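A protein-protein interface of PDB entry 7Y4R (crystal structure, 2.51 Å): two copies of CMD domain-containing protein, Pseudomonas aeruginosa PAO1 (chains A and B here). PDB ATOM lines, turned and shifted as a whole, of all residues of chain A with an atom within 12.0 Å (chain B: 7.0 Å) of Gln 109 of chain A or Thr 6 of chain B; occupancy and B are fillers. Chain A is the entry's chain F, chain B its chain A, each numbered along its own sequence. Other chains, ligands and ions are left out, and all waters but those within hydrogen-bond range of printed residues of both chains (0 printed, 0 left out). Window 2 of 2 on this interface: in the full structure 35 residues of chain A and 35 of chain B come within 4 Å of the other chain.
The backbone carbonyl oxygen of Asn 3 of chain B lies within hydrogen-bond range of the side-chain amide nitrogen of Gln 109 of chain A.
The backbone NH (N) of Trp 5 of chain B is in hydrogen-bond range of the side-chain amide oxygen (OE1) of Gln 109 of chain A (2.9 Å).
Of the 10 printed residues of chain B, 6 touch a printed residue of chain A.
Printed residues of chain B that touch a printed residue of chain A: Asn 3, Asn 4, Trp 5, Thr 6, Val 9 and Leu 72.
No position is printed for both chains.
Of the 13 pairs that touch across the chains among the printed residues, none has its exchanged pair printed and touching as well.
Tyr 99 of chain A touches none of the printed residues of chain B.
Leu 104 of chain A touches none of the printed residues of chain B.
Of the printed residues of chain B, Ala 106 of chain A touches Trp 5 (3.5 Å).
Gln 109 of chain A touches four residues of chain B.
Printed residues of chain B within 4 Å of Phe 110 of chain A: Trp 5 (3.5 Å), Thr 6 (3.8 Å), Val 9 (3.5 Å) and Leu 72 (3.2 Å).
Of the printed residues of chain B, Lys 111 of chain A touches Leu 72.
Trp 5 of chain B touches just these residues of chain A: Arg 102 (3.6 Å), Glu 105 (3.6 Å), Ala 106 (3.5 Å), Gln 109 (2.9 Å) and Phe 110 (3.5 Å).
Of chain A, only Gln 109 (3.6 Å) and Phe 110 (3.8 Å) come within 4 Å of Thr 6 of chain B.
No residue of chain A comes within 4 Å of Glu 7 of chain B.
No residue of chain A comes within 4 Å of Pro 10 of chain B.
The nearest residue of chain B that does not touch Gln 109 of chain A is Glu 7 of chain B (6.2 Å).
The nearest residue of chain A that does not touch Thr 6 of chain B is Ala 106 of chain A (6.2 Å).
The side-chain hydroxyl (OG1) of Thr 6 of chain B is in hydrogen-bond range of the side-chain amide oxygen (OD1) of Asn 4 of chain B, 2.4 Å away.
OE1 of Glu 7 of chain B lies close to ND2 of Asn 4 of chain B (3.5 Å).
Among the printed residues, pairs that only touch across the chains: Phe 110 of chain A with Leu 72 of chain B (3.2 Å), Tyr 107 of chain A with Leu 72 of chain B (3.5 Å), Phe 110 of chain A with Trp 5 of chain B (3.5 Å), Phe 110 of chain A with Val 9 of chain B (3.5 Å), Ala 106 of chain A with Trp 5 of chain B (3.5 Å), Arg 102 of chain A with Trp 5 of chain B (3.6 Å), Glu 105 of chain A with Trp 5 of chain B (3.6 Å), Gln 109 of chain A with Thr 6 of chain B (3.6 Å), Gln 109 of chain A with Asn 4 of chain B (3.7 Å), Lys 111 of chain A with Leu 72 of chain B (3.7 Å) and Phe 110 of chain A with Thr 6 of chain B (3.8 Å).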
ATOM      1  N   VAL A  98       5.573   7.613  25.486  1.00  0.00           N
ATOM      2  CA  VAL A  98       6.099   7.075  26.739  1.00  0.00           C
ATOM      3  C   VAL A  98       7.300   6.173  26.479  1.00  0.00           C
ATOM      4  O   VAL A  98       8.338   6.290  27.140  1.00  0.00           O
ATOM      5  CB  VAL A  98       4.994   6.336  27.514  1.00  0.00           C
ATOM      6  CG1 VAL A  98       5.556   5.747  28.798  1.00  0.00           C
ATOM      7  CG2 VAL A  98       3.854   7.290  27.834  1.00  0.00           C
ATOM      8  N   TYR A  99       7.180   5.259  25.516  1.00  0.00           N
ATOM      9  CA  TYR A  99       8.286   4.359  25.218  1.00  0.00           C
ATOM     10  C   TYR A  99       9.399   5.041  24.437  1.00  0.00           C
ATOM     11  O   TYR A  99      10.540   4.565  24.468  1.00  0.00           O
ATOM     12  CB  TYR A  99       7.775   3.132  24.463  1.00  0.00           C
ATOM     13  CG  TYR A  99       7.157   2.102  25.380  1.00  0.00           C
ATOM     14  CD1 TYR A  99       5.858   2.252  25.847  1.00  0.00           C
ATOM     15  CD2 TYR A  99       7.879   0.992  25.796  1.00  0.00           C
ATOM     16  CE1 TYR A  99       5.291   1.319  26.693  1.00  0.00           C
ATOM     17  CE2 TYR A  99       7.322   0.055  26.643  1.00  0.00           C
ATOM     18  CZ  TYR A  99       6.026   0.223  27.088  1.00  0.00           C
ATOM     19  OH  TYR A  99       5.464  -0.709  27.931  1.00  0.00           O
ATOM     20  N   SER A 100       9.101   6.143  23.744  1.00  0.00           N
ATOM     21  CA  SER A 100      10.166   6.950  23.162  1.00  0.00           C
ATOM     22  C   SER A 100      11.011   7.609  24.244  1.00  0.00           C
ATOM     23  O   SER A 100      12.218   7.798  24.059  1.00  0.00           O
ATOM     24  CB  SER A 100       9.582   8.010  22.228  1.00  0.00           C
ATOM     25  OG  SER A 100       9.113   7.428  21.024  1.00  0.00           O
ATOM     26  N   LEU A 101      10.394   7.964  25.374  1.00  0.00           N
ATOM     27  CA  LEU A 101      11.148   8.526  26.490  1.00  0.00           C
ATOM     28  C   LEU A 101      12.104   7.497  27.079  1.00  0.00           C
ATOM     29  O   LEU A 101      13.200   7.848  27.530  1.00  0.00           O
ATOM     30  CB  LEU A 101      10.190   9.047  27.561  1.00  0.00           C
ATOM     31  CG  LEU A 101       9.417  10.324  27.229  1.00  0.00           C
ATOM     32  CD1 LEU A 101       8.295  10.548  28.231  1.00  0.00           C
ATOM     33  CD2 LEU A 101      10.349  11.524  27.187  1.00  0.00           C
ATOM     34  N   ARG A 102      11.704   6.222  27.089  1.00  0.00           N
ATOM     35  CA  ARG A 102      12.603   5.173  27.558  1.00  0.00           C
ATOM     36  C   ARG A 102      13.805   5.030  26.633  1.00  0.00           C
ATOM     37  O   ARG A 102      14.927   4.788  27.094  1.00  0.00           O
ATOM     38  CB  ARG A 102      11.853   3.846  27.666  1.00  0.00           C
ATOM     39  CG  ARG A 102      10.610   3.891  28.538  1.00  0.00           C
ATOM     40  CD  ARG A 102       9.689   2.724  28.220  1.00  0.00           C
ATOM     41  NE  ARG A 102       8.830   2.367  29.343  1.00  0.00           N
ATOM     42  CZ  ARG A 102       9.214   1.630  30.377  1.00  0.00           C
ATOM     43  NH1 ARG A 102      10.448   1.158  30.469  1.00  0.00           N
ATOM     44  NH2 ARG A 102       8.340   1.360  31.342  1.00  0.00           N
ATOM     45  N   ALA A 103      13.588   5.174  25.322  1.00  0.00           N
ATOM     46  CA  ALA A 103      14.695   5.108  24.377  1.00  0.00           C
ATOM     47  C   ALA A 103      15.652   6.277  24.568  1.00  0.00           C
ATOM     48  O   ALA A 103      16.874   6.103  24.505  1.00  0.00           O
ATOM     49  CB  ALA A 103      14.163   5.074  22.944  1.00  0.00           C
ATOM     50  N   LEU A 104      15.115   7.477  24.801  1.00  0.00           N
ATOM     51  CA  LEU A 104      15.969   8.630  25.062  1.00  0.00           C
ATOM     52  C   LEU A 104      16.707   8.476  26.387  1.00  0.00           C
ATOM     53  O   LEU A 104      17.859   8.908  26.516  1.00  0.00           O
ATOM     54  CB  LEU A 104      15.137   9.911  25.058  1.00  0.00           C
ATOM     55  CG  LEU A 104      14.616  10.384  23.698  1.00  0.00           C
ATOM     56  CD1 LEU A 104      13.644  11.540  23.869  1.00  0.00           C
ATOM     57  CD2 LEU A 104      15.768  10.777  22.787  1.00  0.00           C
ATOM     58  N   GLU A 105      16.060   7.864  27.380  1.00  0.00           N
ATOM     59  CA  GLU A 105      16.718   7.643  28.664  1.00  0.00           C
ATOM     60  C   GLU A 105      17.804   6.581  28.549  1.00  0.00           C
ATOM     61  O   GLU A 105      18.865   6.700  29.174  1.00  0.00           O
ATOM     62  CB  GLU A 105      15.685   7.248  29.720  1.00  0.00           C
ATOM     63  CG  GLU A 105      16.283   6.820  31.051  1.00  0.00           C
ATOM     64  CD  GLU A 105      15.248   6.240  31.995  1.00  0.00           C
ATOM     65  OE1 GLU A 105      14.187   5.791  31.513  1.00  0.00           O
ATOM     66  OE2 GLU A 105      15.495   6.231  33.219  1.00  0.00           O
ATOM     67  N   ALA A 106      17.561   5.537  27.752  1.00  0.00           N
ATOM     68  CA  ALA A 106      18.567   4.496  27.569  1.00  0.00           C
ATOM     69  C   ALA A 106      19.790   5.032  26.837  1.00  0.00           C
ATOM     70  O   ALA A 106      20.927   4.702  27.192  1.00  0.00           O
ATOM     71  CB  ALA A 106      17.965   3.310  26.815  1.00  0.00           C
ATOM     72  N   TYR A 107      19.576   5.863  25.813  1.00  0.00           N
ATOM     73  CA  TYR A 107      20.694   6.442  25.078  1.00  0.00           C
ATOM     74  C   TYR A 107      21.554   7.329  25.967  1.00  0.00           C
ATOM     75  O   TYR A 107      22.775   7.399  25.780  1.00  0.00           O
ATOM     76  CB  TYR A 107      20.175   7.239  23.881  1.00  0.00           C
ATOM     77  CG  TYR A 107      21.259   7.869  23.038  1.00  0.00           C
ATOM     78  CD1 TYR A 107      22.114   7.087  22.273  1.00  0.00           C
ATOM     79  CD2 TYR A 107      21.425   9.248  23.003  1.00  0.00           C
ATOM     80  CE1 TYR A 107      23.101   7.661  21.496  1.00  0.00           C
ATOM     81  CE2 TYR A 107      22.413   9.829  22.231  1.00  0.00           C
ATOM     82  CZ  TYR A 107      23.248   9.031  21.478  1.00  0.00           C
ATOM     83  OH  TYR A 107      24.233   9.604  20.708  1.00  0.00           O
ATOM     84  N   ASP A 108      20.940   8.010  26.938  1.00  0.00           N
ATOM     85  CA  ASP A 108      21.703   8.871  27.834  1.00  0.00           C
ATOM     86  C   ASP A 108      22.573   8.064  28.789  1.00  0.00           C
ATOM     87  O   ASP A 108      23.654   8.521  29.176  1.00  0.00           O
ATOM     88  CB  ASP A 108      20.755   9.779  28.618  1.00  0.00           C
ATOM     89  CG  ASP A 108      21.292  11.187  28.772  1.00  0.00           C
ATOM     90  OD1 ASP A 108      21.668  11.796  27.749  1.00  0.00           O
ATOM     91  OD2 ASP A 108      21.339  11.684  29.917  1.00  0.00           O
ATOM     92  N   GLN A 109      22.126   6.869  29.177  1.00  0.00           N
ATOM     93  CA  GLN A 109      22.897   6.052  30.107  1.00  0.00           C
ATOM     94  C   GLN A 109      24.051   5.333  29.421  1.00  0.00           C
ATOM     95  O   GLN A 109      25.051   5.014  30.074  1.00  0.00           O
ATOM     96  CB  GLN A 109      21.980   5.043  30.801  1.00  0.00           C
ATOM     97  CG  GLN A 109      20.867   5.685  31.614  1.00  0.00           C
ATOM     98  CD  GLN A 109      20.004   4.666  32.333  1.00  0.00           C
ATOM     99  OE1 GLN A 109      20.414   3.525  32.541  1.00  0.00           O
ATOM    100  NE2 GLN A 109      18.801   5.077  32.717  1.00  0.00           N
ATOM    101  N   PHE A 110      23.933   5.066  28.120  1.00  0.00           N
ATOM    102  CA  PHE A 110      25.025   4.467  27.364  1.00  0.00           C
ATOM    103  C   PHE A 110      26.010   5.496  26.831  1.00  0.00           C
ATOM    104  O   PHE A 110      27.134   5.129  26.468  1.00  0.00           O
ATOM    105  CB  PHE A 110      24.476   3.649  26.189  1.00  0.00           C
ATOM    106  CG  PHE A 110      23.686   2.442  26.605  1.00  0.00           C
ATOM    107  CD1 PHE A 110      24.219   1.519  27.490  1.00  0.00           C
ATOM    108  CD2 PHE A 110      22.411   2.227  26.107  1.00  0.00           C
ATOM    109  CE1 PHE A 110      23.494   0.408  27.873  1.00  0.00           C
ATOM    110  CE2 PHE A 110      21.681   1.118  26.487  1.00  0.00           C
ATOM    111  CZ  PHE A 110      22.223   0.207  27.371  1.00  0.00           C
ATOM    112  N   LYS A 111      25.618   6.767  26.781  1.00  0.00           N
ATOM    113  CA  LYS A 111      26.463   7.804  26.206  1.00  0.00           C
ATOM    114  C   LYS A 111      27.720   8.011  27.044  1.00  0.00           C
ATOM    115  O   LYS A 111      27.694   7.912  28.273  1.00  0.00           O
ATOM    116  CB  LYS A 111      25.683   9.115  26.096  1.00  0.00           C
ATOM    117  CG  LYS A 111      26.377  10.201  25.289  1.00  0.00           C
ATOM    118  CD  LYS A 111      25.567  11.492  25.274  1.00  0.00           C
ATOM    119  CE  LYS A 111      24.887  11.744  26.612  1.00  0.00           C
ATOM    120  NZ  LYS A 111      25.810  12.378  27.592  1.00  0.00           N
ATOM    121  N   LYS A 112      28.827   8.297  26.365  1.00  0.00           N
ATOM    122  CA  LYS A 112      30.100   8.546  27.032  1.00  0.00           C
ATOM    123  C   LYS A 112      30.718   9.855  26.553  1.00  0.00           C
ATOM    124  O   LYS A 112      30.026  10.718  26.012  1.00  0.00           O
ATOM    125  CB  LYS A 112      31.068   7.385  26.793  1.00  0.00           C
ATOM    126  CG  LYS A 112      31.144   6.396  27.943  1.00  0.00           C
ATOM    127  CD  LYS A 112      32.415   6.590  28.753  1.00  0.00           C
ATOM    128  CE  LYS A 112      32.459   5.645  29.945  1.00  0.00           C
ATOM    129  NZ  LYS A 112      33.825   5.540  30.528  1.00  0.00           N
ATOM    130  N   ASN B   3      15.249   2.366  34.463  1.00  0.00           N
ATOM    131  CA  ASN B   3      16.088   2.682  35.614  1.00  0.00           C
ATOM    132  C   ASN B   3      17.563   2.464  35.297  1.00  0.00           C
ATOM    133  O   ASN B   3      18.338   3.417  35.224  1.00  0.00           O
ATOM    134  CB  ASN B   3      15.681   1.838  36.824  1.00  0.00           C
ATOM    135  CG  ASN B   3      14.616   2.508  37.670  1.00  0.00           C
ATOM    136  OD1 ASN B   3      14.597   3.731  37.810  1.00  0.00           O
ATOM    137  ND2 ASN B   3      13.723   1.707  38.241  1.00  0.00           N
ATOM    138  N   ASN B   4      17.945   1.205  35.110  1.00  0.00           N
ATOM    139  CA  ASN B   4      19.328   0.823  34.833  1.00  0.00           C
ATOM    140  C   ASN B   4      19.357   0.033  33.526  1.00  0.00           C
ATOM    141  O   ASN B   4      19.309  -1.200  33.529  1.00  0.00           O
ATOM    142  CB  ASN B   4      19.917   0.019  35.993  1.00  0.00           C
ATOM    143  CG  ASN B   4      21.427  -0.089  35.919  1.00  0.00           C
ATOM    144  OD1 ASN B   4      22.065   0.540  35.074  1.00  0.00           O
ATOM    145  ND2 ASN B   4      22.008  -0.879  36.814  1.00  0.00           N
ATOM    146  N   TRP B   5      19.431   0.755  32.405  1.00  0.00           N
ATOM    147  CA  TRP B   5      19.570   0.092  31.113  1.00  0.00           C
ATOM    148  C   TRP B   5      20.951  -0.528  30.951  1.00  0.00           C
ATOM    149  O   TRP B   5      21.110  -1.498  30.200  1.00  0.00           O
ATOM    150  CB  TRP B   5      19.301   1.081  29.980  1.00  0.00           C
ATOM    151  CG  TRP B   5      17.920   1.660  29.994  1.00  0.00           C
ATOM    152  CD1 TRP B   5      17.515   2.796  30.630  1.00  0.00           C
ATOM    153  CD2 TRP B   5      16.761   1.133  29.335  1.00  0.00           C
ATOM    154  NE1 TRP B   5      16.176   3.009  30.411  1.00  0.00           N
ATOM    155  CE2 TRP B   5      15.690   2.003  29.619  1.00  0.00           C
ATOM    156  CE3 TRP B   5      16.527   0.013  28.533  1.00  0.00           C
ATOM    157  CZ2 TRP B   5      14.403   1.785  29.131  1.00  0.00           C
ATOM    158  CZ3 TRP B   5      15.247  -0.202  28.050  1.00  0.00           C
ATOM    159  CH2 TRP B   5      14.203   0.681  28.350  1.00  0.00           C
ATOM    160  N   THR B   6      21.957   0.011  31.645  1.00  0.00           N
ATOM    161  CA  THR B   6      23.308  -0.529  31.559  1.00  0.00           C
ATOM    162  C   THR B   6      23.424  -1.906  32.198  1.00  0.00           C
ATOM    163  O   THR B   6      24.412  -2.606  31.957  1.00  0.00           O
ATOM    164  CB  THR B   6      24.303   0.432  32.211  1.00  0.00           C
ATOM    165  OG1 THR B   6      24.029   0.527  33.614  1.00  0.00           O
ATOM    166  CG2 THR B   6      24.194   1.813  31.583  1.00  0.00           C
ATOM    167  N   GLU B   7      22.450  -2.302  33.018  1.00  0.00           N
ATOM    168  CA  GLU B   7      22.373  -3.654  33.552  1.00  0.00           C
ATOM    169  C   GLU B   7      21.288  -4.493  32.899  1.00  0.00           C
ATOM    170  O   GLU B   7      21.410  -5.719  32.860  1.00  0.00           O
ATOM    171  CB  GLU B   7      22.125  -3.620  35.064  1.00  0.00           C
ATOM    172  CG  GLU B   7      23.147  -4.387  35.886  1.00  0.00           C
ATOM    173  CD  GLU B   7      23.105  -4.017  37.356  1.00  0.00           C
ATOM    174  OE1 GLU B   7      24.101  -3.459  37.860  1.00  0.00           O
ATOM    175  OE2 GLU B   7      22.073  -4.285  38.007  1.00  0.00           O
ATOM    176  N   PHE B   8      20.234  -3.857  32.385  1.00  0.00           N
ATOM    177  CA  PHE B   8      19.156  -4.594  31.735  1.00  0.00           C
ATOM    178  C   PHE B   8      19.612  -5.172  30.402  1.00  0.00           C
ATOM    179  O   PHE B   8      19.346  -6.341  30.096  1.00  0.00           O
ATOM    180  CB  PHE B   8      17.947  -3.677  31.544  1.00  0.00           C
ATOM    181  CG  PHE B   8      16.781  -4.343  30.873  1.00  0.00           C
ATOM    182  CD1 PHE B   8      16.196  -5.471  31.424  1.00  0.00           C
ATOM    183  CD2 PHE B   8      16.267  -3.838  29.690  1.00  0.00           C
ATOM    184  CE1 PHE B   8      15.122  -6.084  30.807  1.00  0.00           C
ATOM    185  CE2 PHE B   8      15.193  -4.445  29.069  1.00  0.00           C
ATOM    186  CZ  PHE B   8      14.619  -5.570  29.628  1.00  0.00           C
ATOM    187  N   VAL B   9      20.309  -4.369  29.596  1.00  0.00           N
ATOM    188  CA  VAL B   9      20.726  -4.823  28.268  1.00  0.00           C
ATOM    189  C   VAL B   9      21.714  -5.987  28.343  1.00  0.00           C
ATOM    190  O   VAL B   9      21.521  -6.977  27.618  1.00  0.00           O
ATOM    191  CB  VAL B   9      21.255  -3.641  27.446  1.00  0.00           C
ATOM    192  CG1 VAL B   9      21.828  -4.120  26.123  1.00  0.00           C
ATOM    193  CG2 VAL B   9      20.148  -2.625  27.213  1.00  0.00           C
ATOM    194  N   PRO B  10      22.771  -5.944  29.164  1.00  0.00           N
ATOM    195  CA  PRO B  10      23.641  -7.129  29.266  1.00  0.00           C
ATOM    196  C   PRO B  10      22.924  -8.357  29.794  1.00  0.00           C
ATOM    197  O   PRO B  10      23.293  -9.482  29.431  1.00  0.00           O
ATOM    198  CB  PRO B  10      24.752  -6.668  30.219  1.00  0.00           C
ATOM    199  CG  PRO B  10      24.764  -5.193  30.095  1.00  0.00           C
ATOM    200  CD  PRO B  10      23.327  -4.809  29.923  1.00  0.00           C
ATOM    201  N   ALA B  11      21.910  -8.180  30.644  1.00  0.00           N
ATOM    202  CA  ALA B  11      21.139  -9.325  31.117  1.00  0.00           C
ATOM    203  C   ALA B  11      20.313  -9.932  29.992  1.00  0.00           C
ATOM    204  O   ALA B  11      20.176 -11.159  29.907  1.00  0.00           O
ATOM    205  CB  ALA B  11      20.242  -8.910  32.282  1.00  0.00           C
ATOM    206  N   LEU B  72      24.054   3.980  19.209  1.00  0.00           N
ATOM    207  CA  LEU B  72      25.156   4.815  19.676  1.00  0.00           C
ATOM    208  C   LEU B  72      26.494   4.298  19.164  1.00  0.00           C
ATOM    209  O   LEU B  72      27.359   5.085  18.759  1.00  0.00           O
ATOM    210  CB  LEU B  72      25.155   4.875  21.202  1.00  0.00           C
ATOM    211  CG  LEU B  72      26.391   5.493  21.860  1.00  0.00           C
ATOM    212  CD1 LEU B  72      26.560   6.950  21.453  1.00  0.00           C
ATOM    213  CD2 LEU B  72      26.306   5.362  23.368  1.00  0.00           C
